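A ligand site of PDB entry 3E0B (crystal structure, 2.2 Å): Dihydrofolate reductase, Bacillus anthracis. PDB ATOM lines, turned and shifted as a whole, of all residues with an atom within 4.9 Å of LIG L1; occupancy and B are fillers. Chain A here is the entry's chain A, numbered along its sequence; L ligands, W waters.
An oxygen (O12) of LIG L1 lies within hydrogen-bond range of the backbone carbonyl oxygen of Asn 24, 3.1 Å away.
An oxygen (O9) of LIG L1 sits at hydrogen-bond distance from the backbone NH (N) of Ala 103, 3.3 Å away.
The backbone NH of Asn 51 sits at hydrogen-bond distance from an oxygen (O2) of LIG L1 (3.0 Å).
N3 of LG2 L2 lies close to N of Val 11 (3.4 Å).
An oxygen (O12) of LIG L1 sits at hydrogen-bond distance from the backbone NH of Asn 24 (3.1 Å).
An oxygen (O2) of LIG L1 sits at hydrogen-bond distance from the backbone NH (N) of Gly 102, 2.8 Å away.
O of Val 11 sits at hydrogen-bond distance from N2 of LG2 L2, 3.3 Å away.
SD of Met 10 lies within hydrogen-bond range of N2 of LG2 L2.
The backbone carbonyl oxygen of Met 10 is in hydrogen-bond range of a nitrogen (N4) of LG2 L2 (2.9 Å).
An oxygen (O17) of LIG L1 lies within hydrogen-bond range of the side-chain hydroxyl of Thr 68, 2.8 Å away.
The backbone carbonyl oxygen (O) of Ala 12 is in hydrogen-bond range of a nitrogen (N7) of LIG L1 (2.8 Å).
An oxygen (O14) of LIG L1 sits at hydrogen-bond distance from the backbone NH (N) of Ala 12, at 2.9 Å.
O of Phe 100 sits at hydrogen-bond distance from N4 of LG2 L2 (3.4 Å).
N of Ile 105 sits at hydrogen-bond distance from O1 of LIG L1, 3.1 Å away.
An oxygen (O3) of LIG L1 is in hydrogen-bond range of the backbone NH of Lys 50 (3.5 Å).
O17 of LIG L1 lies within salt-bridge range of NE of Arg 49.
O of Ile 19 sits close to N7 of LIG L1.
An oxygen (O9) of LIG L1 is in hydrogen-bond range of the backbone NH of Gln 104 (3.0 Å).
N of Arg 69 lies within hydrogen-bond range of O15 of LIG L1 (3.0 Å).
A nitrogen (N4) of LG2 L2 sits close to an oxygen (O14) of LIG L1 (3.4 Å).
The side-chain hydroxyl of Tyr 106 lies within hydrogen-bond range of the backbone carbonyl oxygen of Met 10 (2.6 Å).
O of Phe 100 sits at hydrogen-bond distance from ND2 of Asn 51.
N of Thr 129 sits at hydrogen-bond distance from O of Gly 20 (3.2 Å).
A ring nitrogen (NE2) of His 82 is in hydrogen-bond range of the backbone carbonyl oxygen of Asn 70 (3.2 Å).
OG1 of Thr 68 lies within hydrogen-bond range of N of Asn 70 (2.9 Å).
N of Ile 19 is in hydrogen-bond range of O of Thr 129.
O of Val 67 is in hydrogen-bond range of N of Arg 49 (3.0 Å).
ND2 of Asn 51 sits at hydrogen-bond distance from O of Gly 101.
Merely in contact with LIG L1: Phe 100 (3.2 Å), Gly 48 (3.2 Å), Val 67 (3.3 Å), Asn 23 (3.3 Å), His 82 (3.4 Å), Val 11 (3.5 Å), Leu 25 (3.5 Å), Trp 27 (3.5 Å), Leu 108 (3.5 Å), Gly 20 (3.7 Å), Gly 101 (3.7 Å), Tyr 106 (3.7 Å), Thr 129 (3.8 Å) and Asn 70 (3.9 Å).
Of the 30 residues printed, 26 come within 4 Å of LIG L1.
The nearest printed residue that does not touch LIG L1 is Lys 21 (4.04 Å).
Water W3 lies within hydrogen-bond range of O13 of LIG L1, OD1 of Asn 51 and O2 of LG2 L2.
Water W2 bridges N2 of LIG L1 (2.7 Å) and NH2 of Arg 69 (3.5 Å).
Water W4 bridges O17 of LIG L1 (2.7 Å) and OD1 of Asn 70 (3.3 Å).
Water W6 lies within hydrogen-bond range of the guanidinium group (NH1) of Arg 69 and an oxygen (O15) of LIG L1.
Water W1 lies within hydrogen-bond range of a nitrogen (N4) of LIG L1 (3.0 Å) and the backbone carbonyl oxygen of His 82 (3.2 Å).
Water W5 lies within hydrogen-bond range of N of Asn 23 (2.6 Å), OG1 of Thr 129 (3.2 Å) and O12 of LIG L1 (3.3 Å).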
ATOM      1  N   MET A  10     -12.205 -25.101   1.092  1.00  0.00           N
ATOM      2  CA  MET A  10     -11.425 -24.365   0.117  1.00  0.00           C
ATOM      3  C   MET A  10     -10.957 -23.062   0.751  1.00  0.00           C
ATOM      4  O   MET A  10     -11.756 -22.175   1.046  1.00  0.00           O
ATOM      5  CB  MET A  10     -12.223 -24.140  -1.166  1.00  0.00           C
ATOM      6  CG  MET A  10     -11.543 -23.245  -2.217  1.00  0.00           C
ATOM      7  SD  MET A  10      -9.960 -23.793  -2.918  1.00  0.00           S
ATOM      8  CE  MET A  10     -10.445 -25.215  -3.915  1.00  0.00           C
ATOM      9  N   VAL A  11      -9.633 -22.952   0.934  1.00  0.00           N
ATOM     10  CA  VAL A  11      -9.070 -21.802   1.649  1.00  0.00           C
ATOM     11  C   VAL A  11      -7.643 -21.445   1.230  1.00  0.00           C
ATOM     12  O   VAL A  11      -6.872 -22.287   0.756  1.00  0.00           O
ATOM     13  CB  VAL A  11      -9.150 -22.022   3.212  1.00  0.00           C
ATOM     14  CG1 VAL A  11      -8.205 -23.124   3.652  1.00  0.00           C
ATOM     15  CG2 VAL A  11      -8.859 -20.733   3.976  1.00  0.00           C
ATOM     16  N   ALA A  12      -7.312 -20.160   1.372  1.00  0.00           N
ATOM     17  CA  ALA A  12      -5.959 -19.656   1.139  1.00  0.00           C
ATOM     18  C   ALA A  12      -5.547 -18.868   2.393  1.00  0.00           C
ATOM     19  O   ALA A  12      -6.287 -17.981   2.858  1.00  0.00           O
ATOM     20  CB  ALA A  12      -5.947 -18.761  -0.079  1.00  0.00           C
ATOM     21  N   ILE A  19      -6.426 -15.139   6.893  1.00  0.00           N
ATOM     22  CA  ILE A  19      -7.223 -15.271   5.693  1.00  0.00           C
ATOM     23  C   ILE A  19      -7.955 -13.960   5.343  1.00  0.00           C
ATOM     24  O   ILE A  19      -8.433 -13.798   4.222  1.00  0.00           O
ATOM     25  CB  ILE A  19      -8.274 -16.462   5.753  1.00  0.00           C
ATOM     26  CG1 ILE A  19      -9.434 -16.143   6.722  1.00  0.00           C
ATOM     27  CG2 ILE A  19      -7.568 -17.844   6.059  1.00  0.00           C
ATOM     28  CD1 ILE A  19     -10.443 -17.277   6.872  1.00  0.00           C
ATOM     29  N   GLY A  20      -7.967 -13.012   6.269  1.00  0.00           N
ATOM     30  CA  GLY A  20      -8.671 -11.766   6.017  1.00  0.00           C
ATOM     31  C   GLY A  20      -8.197 -10.552   6.811  1.00  0.00           C
ATOM     32  O   GLY A  20      -7.558 -10.681   7.853  1.00  0.00           O
ATOM     33  N   LYS A  21      -8.574  -9.379   6.305  1.00  0.00           N
ATOM     34  CA  LYS A  21      -8.231  -8.105   6.921  1.00  0.00           C
ATOM     35  C   LYS A  21      -9.283  -7.088   6.509  1.00  0.00           C
ATOM     36  O   LYS A  21      -9.592  -6.957   5.319  1.00  0.00           O
ATOM     37  CB  LYS A  21      -6.839  -7.629   6.492  1.00  0.00           C
ATOM     38  CG  LYS A  21      -6.449  -6.266   7.043  1.00  0.00           C
ATOM     39  CD  LYS A  21      -5.150  -5.798   6.426  1.00  0.00           C
ATOM     40  CE  LYS A  21      -5.042  -4.260   6.402  1.00  0.00           C
ATOM     41  NZ  LYS A  21      -6.083  -3.613   5.506  1.00  0.00           N
ATOM     42  N   ASN A  23     -12.457  -7.169   6.730  1.00  0.00           N
ATOM     43  CA  ASN A  23     -13.562  -7.777   5.982  1.00  0.00           C
ATOM     44  C   ASN A  23     -13.274  -7.928   4.465  1.00  0.00           C
ATOM     45  O   ASN A  23     -14.169  -7.870   3.641  1.00  0.00           O
ATOM     46  CB  ASN A  23     -14.859  -7.003   6.241  1.00  0.00           C
ATOM     47  CG  ASN A  23     -16.085  -7.836   6.002  1.00  0.00           C
ATOM     48  OD1 ASN A  23     -16.104  -9.040   6.252  1.00  0.00           O
ATOM     49  ND2 ASN A  23     -17.145  -7.186   5.522  1.00  0.00           N
ATOM     50  N   ASN A  24     -12.000  -8.170   4.128  1.00  0.00           N
ATOM     51  CA  ASN A  24     -11.575  -8.402   2.747  1.00  0.00           C
ATOM     52  C   ASN A  24     -10.338  -9.313   2.737  1.00  0.00           C
ATOM     53  O   ASN A  24      -9.877  -9.779   3.797  1.00  0.00           O
ATOM     54  CB  ASN A  24     -11.235  -7.055   2.093  1.00  0.00           C
ATOM     55  CG  ASN A  24     -11.402  -7.056   0.547  1.00  0.00           C
ATOM     56  OD1 ASN A  24     -11.128  -8.051  -0.126  1.00  0.00           O
ATOM     57  ND2 ASN A  24     -11.796  -5.904   0.000  1.00  0.00           N
ATOM     58  N   LEU A  25      -9.834  -9.580   1.549  1.00  0.00           N
ATOM     59  CA  LEU A  25      -8.607 -10.380   1.334  1.00  0.00           C
ATOM     60  C   LEU A  25      -7.353  -9.495   1.517  1.00  0.00           C
ATOM     61  O   LEU A  25      -7.332  -8.363   1.040  1.00  0.00           O
ATOM     62  CB  LEU A  25      -8.625 -10.914  -0.098  1.00  0.00           C
ATOM     63  CG  LEU A  25      -9.105 -12.346  -0.383  1.00  0.00           C
ATOM     64  CD1 LEU A  25      -9.810 -13.047   0.804  1.00  0.00           C
ATOM     65  CD2 LEU A  25      -9.914 -12.398  -1.686  1.00  0.00           C
ATOM     66  N   TRP A  27      -4.464 -10.005   0.146  1.00  0.00           N
ATOM     67  CA  TRP A  27      -3.581 -10.130  -1.015  1.00  0.00           C
ATOM     68  C   TRP A  27      -4.405 -10.227  -2.280  1.00  0.00           C
ATOM     69  O   TRP A  27      -5.598 -10.519  -2.231  1.00  0.00           O
ATOM     70  CB  TRP A  27      -2.733 -11.415  -0.896  1.00  0.00           C
ATOM     71  CG  TRP A  27      -3.590 -12.648  -0.644  1.00  0.00           C
ATOM     72  CD1 TRP A  27      -4.321 -13.342  -1.573  1.00  0.00           C
ATOM     73  CD2 TRP A  27      -3.823 -13.288   0.618  1.00  0.00           C
ATOM     74  NE1 TRP A  27      -4.992 -14.389  -0.966  1.00  0.00           N
ATOM     75  CE2 TRP A  27      -4.681 -14.382   0.377  1.00  0.00           C
ATOM     76  CE3 TRP A  27      -3.386 -13.045   1.933  1.00  0.00           C
ATOM     77  CZ2 TRP A  27      -5.120 -15.241   1.410  1.00  0.00           C
ATOM     78  CZ3 TRP A  27      -3.816 -13.903   2.955  1.00  0.00           C
ATOM     79  CH2 TRP A  27      -4.691 -14.969   2.685  1.00  0.00           C
ATOM     80  N   GLY A  48     -20.090 -17.938   4.560  1.00  0.00           N
ATOM     81  CA  GLY A  48     -20.653 -17.162   5.665  1.00  0.00           C
ATOM     82  C   GLY A  48     -21.263 -15.923   5.064  1.00  0.00           C
ATOM     83  O   GLY A  48     -20.849 -15.511   3.990  1.00  0.00           O
ATOM     84  N   ARG A  49     -22.223 -15.317   5.761  1.00  0.00           N
ATOM     85  CA  ARG A  49     -22.893 -14.112   5.272  1.00  0.00           C
ATOM     86  C   ARG A  49     -21.906 -12.969   4.971  1.00  0.00           C
ATOM     87  O   ARG A  49     -22.005 -12.298   3.938  1.00  0.00           O
ATOM     88  CB  ARG A  49     -23.994 -13.691   6.240  1.00  0.00           C
ATOM     89  CG  ARG A  49     -24.965 -12.631   5.706  1.00  0.00           C
ATOM     90  CD  ARG A  49     -24.502 -11.215   6.030  1.00  0.00           C
ATOM     91  NE  ARG A  49     -24.376 -10.987   7.470  1.00  0.00           N
ATOM     92  CZ  ARG A  49     -23.784  -9.916   8.004  1.00  0.00           C
ATOM     93  NH1 ARG A  49     -23.288  -8.961   7.219  1.00  0.00           N
ATOM     94  NH2 ARG A  49     -23.662  -9.813   9.325  1.00  0.00           N
ATOM     95  N   LYS A  50     -20.922 -12.783   5.846  1.00  0.00           N
ATOM     96  CA  LYS A  50     -19.892 -11.753   5.642  1.00  0.00           C
ATOM     97  C   LYS A  50     -19.045 -12.048   4.423  1.00  0.00           C
ATOM     98  O   LYS A  50     -18.877 -11.182   3.574  1.00  0.00           O
ATOM     99  CB  LYS A  50     -19.031 -11.568   6.887  1.00  0.00           C
ATOM    100  CG  LYS A  50     -19.727 -10.793   7.970  1.00  0.00           C
ATOM    101  CD  LYS A  50     -18.759 -10.192   8.942  1.00  0.00           C
ATOM    102  CE  LYS A  50     -19.487  -9.827  10.249  1.00  0.00           C
ATOM    103  NZ  LYS A  50     -18.576  -9.224  11.295  1.00  0.00           N
ATOM    104  N   ASN A  51     -18.534 -13.277   4.320  1.00  0.00           N
ATOM    105  CA  ASN A  51     -17.802 -13.643   3.105  1.00  0.00           C
ATOM    106  C   ASN A  51     -18.653 -13.316   1.868  1.00  0.00           C
ATOM    107  O   ASN A  51     -18.198 -12.623   0.970  1.00  0.00           O
ATOM    108  CB  ASN A  51     -17.404 -15.121   3.095  1.00  0.00           C
ATOM    109  CG  ASN A  51     -16.637 -15.498   1.835  1.00  0.00           C
ATOM    110  OD1 ASN A  51     -15.991 -14.644   1.222  1.00  0.00           O
ATOM    111  ND2 ASN A  51     -16.748 -16.756   1.409  1.00  0.00           N
ATOM    112  N   ALA A  54     -18.832  -9.584   0.925  1.00  0.00           N
ATOM    113  CA  ALA A  54     -17.567  -9.065   0.446  1.00  0.00           C
ATOM    114  C   ALA A  54     -17.379  -9.429  -1.047  1.00  0.00           C
ATOM    115  O   ALA A  54     -16.962  -8.598  -1.839  1.00  0.00           O
ATOM    116  CB  ALA A  54     -16.406  -9.569   1.293  1.00  0.00           C
ATOM    117  N   VAL A  67     -24.765 -18.833   4.537  1.00  0.00           N
ATOM    118  CA  VAL A  67     -25.099 -19.177   5.929  1.00  0.00           C
ATOM    119  C   VAL A  67     -25.281 -17.926   6.781  1.00  0.00           C
ATOM    120  O   VAL A  67     -24.401 -17.067   6.843  1.00  0.00           O
ATOM    121  CB  VAL A  67     -24.069 -20.144   6.561  1.00  0.00           C
ATOM    122  CG1 VAL A  67     -24.578 -20.662   7.959  1.00  0.00           C
ATOM    123  CG2 VAL A  67     -23.819 -21.297   5.617  1.00  0.00           C
ATOM    124  N   THR A  68     -26.459 -17.820   7.408  1.00  0.00           N
ATOM    125  CA  THR A  68     -26.821 -16.678   8.220  1.00  0.00           C
ATOM    126  C   THR A  68     -27.800 -17.111   9.339  1.00  0.00           C
ATOM    127  O   THR A  68     -28.505 -18.098   9.189  1.00  0.00           O
ATOM    128  CB  THR A  68     -27.442 -15.511   7.345  1.00  0.00           C
ATOM    129  OG1 THR A  68     -27.999 -14.502   8.203  1.00  0.00           O
ATOM    130  CG2 THR A  68     -28.562 -16.016   6.432  1.00  0.00           C
ATOM    131  N   ARG A  69     -27.783 -16.407  10.469  1.00  0.00           N
ATOM    132  CA  ARG A  69     -28.779 -16.640  11.517  1.00  0.00           C
ATOM    133  C   ARG A  69     -30.027 -15.781  11.282  1.00  0.00           C
ATOM    134  O   ARG A  69     -31.014 -15.907  12.004  1.00  0.00           O
ATOM    135  CB  ARG A  69     -28.210 -16.335  12.903  1.00  0.00           C
ATOM    136  CG  ARG A  69     -27.132 -17.311  13.410  1.00  0.00           C
ATOM    137  CD  ARG A  69     -26.825 -16.988  14.872  1.00  0.00           C
ATOM    138  NE  ARG A  69     -25.677 -17.726  15.406  1.00  0.00           N
ATOM    139  CZ  ARG A  69     -24.410 -17.322  15.305  1.00  0.00           C
ATOM    140  NH1 ARG A  69     -24.098 -16.203  14.650  1.00  0.00           N
ATOM    141  NH2 ARG A  69     -23.446 -18.049  15.832  1.00  0.00           N
ATOM    142  N   ASN A  70     -29.969 -14.924  10.267  1.00  0.00           N
ATOM    143  CA  ASN A  70     -31.081 -14.025   9.889  1.00  0.00           C
ATOM    144  C   ASN A  70     -32.141 -14.784   9.076  1.00  0.00           C
ATOM    145  O   ASN A  70     -31.907 -15.146   7.915  1.00  0.00           O
ATOM    146  CB  ASN A  70     -30.509 -12.858   9.061  1.00  0.00           C
ATOM    147  CG  ASN A  70     -31.494 -11.679   8.864  1.00  0.00           C
ATOM    148  OD1 ASN A  70     -31.054 -10.544   8.712  1.00  0.00           O
ATOM    149  ND2 ASN A  70     -32.786 -11.953   8.811  1.00  0.00           N
ATOM    150  N   HIS A  82     -29.494 -21.682   7.552  1.00  0.00           N
ATOM    151  CA  HIS A  82     -29.322 -21.086   8.847  1.00  0.00           C
ATOM    152  C   HIS A  82     -28.637 -22.012   9.824  1.00  0.00           C
ATOM    153  O   HIS A  82     -28.554 -21.695  11.004  1.00  0.00           O
ATOM    154  CB  HIS A  82     -30.661 -20.599   9.402  1.00  0.00           C
ATOM    155  CG  HIS A  82     -31.440 -19.750   8.436  1.00  0.00           C
ATOM    156  ND1 HIS A  82     -32.312 -20.297   7.516  1.00  0.00           N
ATOM    157  CD2 HIS A  82     -31.383 -18.422   8.162  1.00  0.00           C
ATOM    158  CE1 HIS A  82     -32.825 -19.332   6.773  1.00  0.00           C
ATOM    159  NE2 HIS A  82     -32.257 -18.194   7.124  1.00  0.00           N
ATOM    160  N   SER A  83     -28.082 -23.114   9.316  1.00  0.00           N
ATOM    161  CA  SER A  83     -27.431 -24.130  10.162  1.00  0.00           C
ATOM    162  C   SER A  83     -26.706 -25.165   9.316  1.00  0.00           C
ATOM    163  O   SER A  83     -27.010 -25.339   8.136  1.00  0.00           O
ATOM    164  CB  SER A  83     -28.496 -24.874  11.031  1.00  0.00           C
ATOM    165  OG  SER A  83     -29.450 -25.563  10.207  1.00  0.00           O
ATOM    166  N   PHE A 100     -16.360 -22.474   1.765  1.00  0.00           N
ATOM    167  CA  PHE A 100     -15.614 -21.436   1.126  1.00  0.00           C
ATOM    168  C   PHE A 100     -15.296 -20.256   2.056  1.00  0.00           C
ATOM    169  O   PHE A 100     -14.834 -19.190   1.602  1.00  0.00           O
ATOM    170  CB  PHE A 100     -16.462 -20.990  -0.056  1.00  0.00           C
ATOM    171  CG  PHE A 100     -15.714 -20.310  -1.149  1.00  0.00           C
ATOM    172  CD1 PHE A 100     -14.742 -20.986  -1.858  1.00  0.00           C
ATOM    173  CD2 PHE A 100     -16.128 -19.048  -1.596  1.00  0.00           C
ATOM    174  CE1 PHE A 100     -14.090 -20.368  -2.940  1.00  0.00           C
ATOM    175  CE2 PHE A 100     -15.489 -18.425  -2.661  1.00  0.00           C
ATOM    176  CZ  PHE A 100     -14.461 -19.098  -3.345  1.00  0.00           C
ATOM    177  N   GLY A 101     -15.546 -20.423   3.365  1.00  0.00           N
ATOM    178  CA  GLY A 101     -15.252 -19.381   4.365  1.00  0.00           C
ATOM    179  C   GLY A 101     -16.379 -18.392   4.654  1.00  0.00           C
ATOM    180  O   GLY A 101     -17.456 -18.478   4.055  1.00  0.00           O
ATOM    181  N   GLY A 102     -16.113 -17.398   5.513  1.00  0.00           N
ATOM    182  CA  GLY A 102     -14.818 -17.223   6.154  1.00  0.00           C
ATOM    183  C   GLY A 102     -14.638 -18.001   7.430  1.00  0.00           C
ATOM    184  O   GLY A 102     -15.140 -19.119   7.563  1.00  0.00           O
ATOM    185  N   ALA A 103     -13.978 -17.397   8.406  1.00  0.00           N
ATOM    186  CA  ALA A 103     -13.571 -18.090   9.614  1.00  0.00           C
ATOM    187  C   ALA A 103     -14.689 -18.687  10.479  1.00  0.00           C
ATOM    188  O   ALA A 103     -14.531 -19.809  10.971  1.00  0.00           O
ATOM    189  CB  ALA A 103     -12.628 -17.217  10.442  1.00  0.00           C
ATOM    190  N   GLN A 104     -15.762 -17.942  10.694  1.00  0.00           N
ATOM    191  CA  GLN A 104     -16.884 -18.474  11.480  1.00  0.00           C
ATOM    192  C   GLN A 104     -17.474 -19.690  10.803  1.00  0.00           C
ATOM    193  O   GLN A 104     -17.743 -20.707  11.446  1.00  0.00           O
ATOM    194  CB  GLN A 104     -17.967 -17.432  11.709  1.00  0.00           C
ATOM    195  CG  GLN A 104     -17.526 -16.264  12.563  1.00  0.00           C
ATOM    196  CD  GLN A 104     -18.673 -15.342  12.913  1.00  0.00           C
ATOM    197  OE1 GLN A 104     -18.579 -14.141  12.729  1.00  0.00           O
ATOM    198  NE2 GLN A 104     -19.740 -15.892  13.417  1.00  0.00           N
ATOM    199  N   ILE A 105     -17.622 -19.610   9.475  1.00  0.00           N
ATOM    200  CA  ILE A 105     -18.126 -20.741   8.682  1.00  0.00           C
ATOM    201  C   ILE A 105     -17.170 -21.930   8.640  1.00  0.00           C
ATOM    202  O   ILE A 105     -17.619 -23.091   8.676  1.00  0.00           O
ATOM    203  CB  ILE A 105     -18.592 -20.288   7.286  1.00  0.00           C
ATOM    204  CG1 ILE A 105     -20.122 -20.153   7.274  1.00  0.00           C
ATOM    205  CG2 ILE A 105     -18.199 -21.289   6.247  1.00  0.00           C
ATOM    206  CD1 ILE A 105     -20.690 -19.350   8.449  1.00  0.00           C
ATOM    207  N   TYR A 106     -15.853 -21.659   8.596  1.00  0.00           N
ATOM    208  CA  TYR A 106     -14.877 -22.751   8.685  1.00  0.00           C
ATOM    209  C   TYR A 106     -14.979 -23.455  10.026  1.00  0.00           C
ATOM    210  O   TYR A 106     -14.881 -24.677  10.079  1.00  0.00           O
ATOM    211  CB  TYR A 106     -13.427 -22.256   8.491  1.00  0.00           C
ATOM    212  CG  TYR A 106     -13.082 -21.861   7.066  1.00  0.00           C
ATOM    213  CD1 TYR A 106     -13.377 -22.688   5.990  1.00  0.00           C
ATOM    214  CD2 TYR A 106     -12.377 -20.693   6.816  1.00  0.00           C
ATOM    215  CE1 TYR A 106     -13.057 -22.334   4.713  1.00  0.00           C
ATOM    216  CE2 TYR A 106     -12.058 -20.324   5.540  1.00  0.00           C
ATOM    217  CZ  TYR A 106     -12.387 -21.155   4.491  1.00  0.00           C
ATOM    218  OH  TYR A 106     -12.059 -20.785   3.203  1.00  0.00           O
ATOM    219  N   LEU A 108     -17.642 -23.597  11.957  1.00  0.00           N
ATOM    220  CA  LEU A 108     -18.909 -24.339  11.962  1.00  0.00           C
ATOM    221  C   LEU A 108     -18.760 -25.733  11.388  1.00  0.00           C
ATOM    222  O   LEU A 108     -19.258 -26.705  11.964  1.00  0.00           O
ATOM    223  CB  LEU A 108     -19.985 -23.617  11.124  1.00  0.00           C
ATOM    224  CG  LEU A 108     -21.207 -22.954  11.747  1.00  0.00           C
ATOM    225  CD1 LEU A 108     -22.213 -22.676  10.646  1.00  0.00           C
ATOM    226  CD2 LEU A 108     -21.854 -23.828  12.868  1.00  0.00           C
ATOM    227  N   THR A 129      -8.581 -11.935  10.601  1.00  0.00           N
ATOM    228  CA  THR A 129      -9.345 -13.196  10.493  1.00  0.00           C
ATOM    229  C   THR A 129      -8.395 -14.365  10.180  1.00  0.00           C
ATOM    230  O   THR A 129      -7.500 -14.242   9.350  1.00  0.00           O
ATOM    231  CB  THR A 129     -10.529 -13.079   9.467  1.00  0.00           C
ATOM    232  OG1 THR A 129     -11.291 -11.913   9.765  1.00  0.00           O
ATOM    233  CG2 THR A 129     -11.487 -14.287   9.571  1.00  0.00           C
HETATM  234  P1  LIG L   1     -18.029 -15.399   7.789  1.00  0.00           P
HETATM  235  O1  LIG L   1     -17.673 -16.649   8.488  1.00  0.00           O
HETATM  236  O2  LIG L   1     -17.984 -15.495   6.302  1.00  0.00           O
HETATM  237  O3  LIG L   1     -19.522 -14.994   8.138  1.00  0.00           O
HETATM  238  C1  LIG L   1     -19.914 -14.858   9.466  1.00  0.00           C
HETATM  239  C2  LIG L   1     -21.418 -14.832   9.377  1.00  0.00           C
HETATM  240  O4  LIG L   1     -21.871 -16.158   9.165  1.00  0.00           O
HETATM  241  C3  LIG L   1     -22.106 -14.358  10.642  1.00  0.00           C
HETATM  242  O5  LIG L   1     -22.201 -12.968  10.675  1.00  0.00           O
HETATM  243  C4  LIG L   1     -23.453 -15.030  10.518  1.00  0.00           C
HETATM  244  O6  LIG L   1     -24.288 -14.273   9.646  1.00  0.00           O
HETATM  245  C5  LIG L   1     -23.098 -16.338   9.805  1.00  0.00           C
HETATM  246  N1  LIG L   1     -22.930 -17.359  10.832  1.00  0.00           N
HETATM  247  C6  LIG L   1     -21.841 -17.569  11.643  1.00  0.00           C
HETATM  248  N2  LIG L   1     -22.102 -18.638  12.441  1.00  0.00           N
HETATM  249  C7  LIG L   1     -23.347 -19.088  12.143  1.00  0.00           C
HETATM  250  C8  LIG L   1     -24.130 -20.111  12.665  1.00  0.00           C
HETATM  251  N3  LIG L   1     -23.667 -20.879  13.642  1.00  0.00           N
HETATM  252  N4  LIG L   1     -25.395 -20.329  12.134  1.00  0.00           N
HETATM  253  C9  LIG L   1     -25.889 -19.548  11.116  1.00  0.00           C
HETATM  254  N5  LIG L   1     -25.111 -18.533  10.617  1.00  0.00           N
HETATM  255  C10 LIG L   1     -23.875 -18.294  11.135  1.00  0.00           C
HETATM  256  O7  LIG L   1     -17.240 -14.135   8.436  1.00  0.00           O
HETATM  257  P2  LIG L   1     -15.751 -13.905   9.051  1.00  0.00           P
HETATM  258  O8  LIG L   1     -15.629 -12.514   9.539  1.00  0.00           O
HETATM  259  O9  LIG L   1     -15.498 -14.983  10.005  1.00  0.00           O
HETATM  260  O10 LIG L   1     -14.801 -14.128   7.729  1.00  0.00           O
HETATM  261  C11 LIG L   1     -14.826 -13.204   6.654  1.00  0.00           C
HETATM  262  C12 LIG L   1     -13.406 -12.777   6.289  1.00  0.00           C
HETATM  263  O11 LIG L   1     -12.640 -13.853   5.785  1.00  0.00           O
HETATM  264  C13 LIG L   1     -13.358 -11.707   5.210  1.00  0.00           C
HETATM  265  O12 LIG L   1     -12.213 -10.923   5.490  1.00  0.00           O
HETATM  266  C14 LIG L   1     -13.058 -12.481   3.954  1.00  0.00           C
HETATM  267  O13 LIG L   1     -12.507 -11.631   2.989  1.00  0.00           O
HETATM  268  C15 LIG L   1     -12.096 -13.542   4.500  1.00  0.00           C
HETATM  269  N6  LIG L   1     -12.072 -14.789   3.704  1.00  0.00           N
HETATM  270  C16 LIG L   1     -10.861 -15.288   3.282  1.00  0.00           C
HETATM  271  C17 LIG L   1     -10.819 -16.494   2.575  1.00  0.00           C
HETATM  272  C18 LIG L   1      -9.517 -17.035   2.086  1.00  0.00           C
HETATM  273  O14 LIG L   1      -9.498 -18.325   1.544  1.00  0.00           O
HETATM  274  N7  LIG L   1      -8.402 -16.306   2.196  1.00  0.00           N
HETATM  275  C19 LIG L   1     -12.007 -17.189   2.313  1.00  0.00           C
HETATM  276  C20 LIG L   1     -13.223 -16.684   2.741  1.00  0.00           C
HETATM  277  C21 LIG L   1     -13.240 -15.476   3.449  1.00  0.00           C
HETATM  278  P3  LIG L   1     -25.365 -13.201  10.159  1.00  0.00           P
HETATM  279  O15 LIG L   1     -26.305 -13.877  11.157  1.00  0.00           O
HETATM  280  O16 LIG L   1     -24.583 -12.108  10.824  1.00  0.00           O
HETATM  281  O17 LIG L   1     -26.081 -12.635   8.980  1.00  0.00           O
HETATM  282  C1  LG2 L   2      -8.300 -15.696  -1.957  1.00  0.00           C
HETATM  283  C2  LG2 L   2      -9.212 -16.480  -2.863  1.00  0.00           C
HETATM  284  C3  LG2 L   2      -9.544 -17.826  -2.202  1.00  0.00           C
HETATM  285  N1  LG2 L   2      -8.683 -18.834  -2.376  1.00  0.00           N
HETATM  286  C4  LG2 L   2      -8.912 -20.064  -1.870  1.00  0.00           C
HETATM  287  N2  LG2 L   2      -7.999 -21.032  -2.081  1.00  0.00           N
HETATM  288  N3  LG2 L   2     -10.028 -20.304  -1.157  1.00  0.00           N
HETATM  289  C5  LG2 L   2     -10.926 -19.335  -0.934  1.00  0.00           C
HETATM  290  N4  LG2 L   2     -12.044 -19.595  -0.250  1.00  0.00           N
HETATM  291  C6  LG2 L   2     -10.710 -18.055  -1.474  1.00  0.00           C
HETATM  292  C7  LG2 L   2     -11.650 -16.968  -1.284  1.00  0.00           C
HETATM  293  C8  LG2 L   2     -12.409 -15.967  -1.193  1.00  0.00           C
HETATM  294  C9  LG2 L   2     -13.240 -14.744  -1.070  1.00  0.00           C
HETATM  295  C10 LG2 L   2     -13.492 -14.053  -2.427  1.00  0.00           C
HETATM  296  C11 LG2 L   2     -13.733 -14.840  -3.574  1.00  0.00           C
HETATM  297  C12 LG2 L   2     -13.989 -14.244  -4.824  1.00  0.00           C
HETATM  298  O1  LG2 L   2     -14.233 -14.989  -5.971  1.00  0.00           O
HETATM  299  C13 LG2 L   2     -14.221 -16.404  -5.765  1.00  0.00           C
HETATM  300  C14 LG2 L   2     -14.020 -12.862  -4.921  1.00  0.00           C
HETATM  301  C15 LG2 L   2     -13.795 -12.075  -3.786  1.00  0.00           C
HETATM  302  C16 LG2 L   2     -13.548 -12.658  -2.542  1.00  0.00           C
HETATM  303  O2  LG2 L   2     -13.342 -11.879  -1.414  1.00  0.00           O
HETATM  304  C17 LG2 L   2     -13.585 -10.480  -1.566  1.00  0.00           C
HETATM  305  O   HOH W   1     -26.719 -22.616  13.483  1.00  0.00           O
HETATM  306  O   HOH W   2     -20.669 -19.630  14.513  1.00  0.00           O
HETATM  307  O   HOH W   3     -14.438 -12.320   1.255  1.00  0.00           O
HETATM  308  O   HOH W   4     -27.766 -10.529   8.592  1.00  0.00           O
HETATM  309  O   HOH W   5     -11.591  -9.108   8.179  1.00  0.00           O
HETATM  310  O   HOH W   6     -25.399 -14.041  13.748  1.00  0.00           O
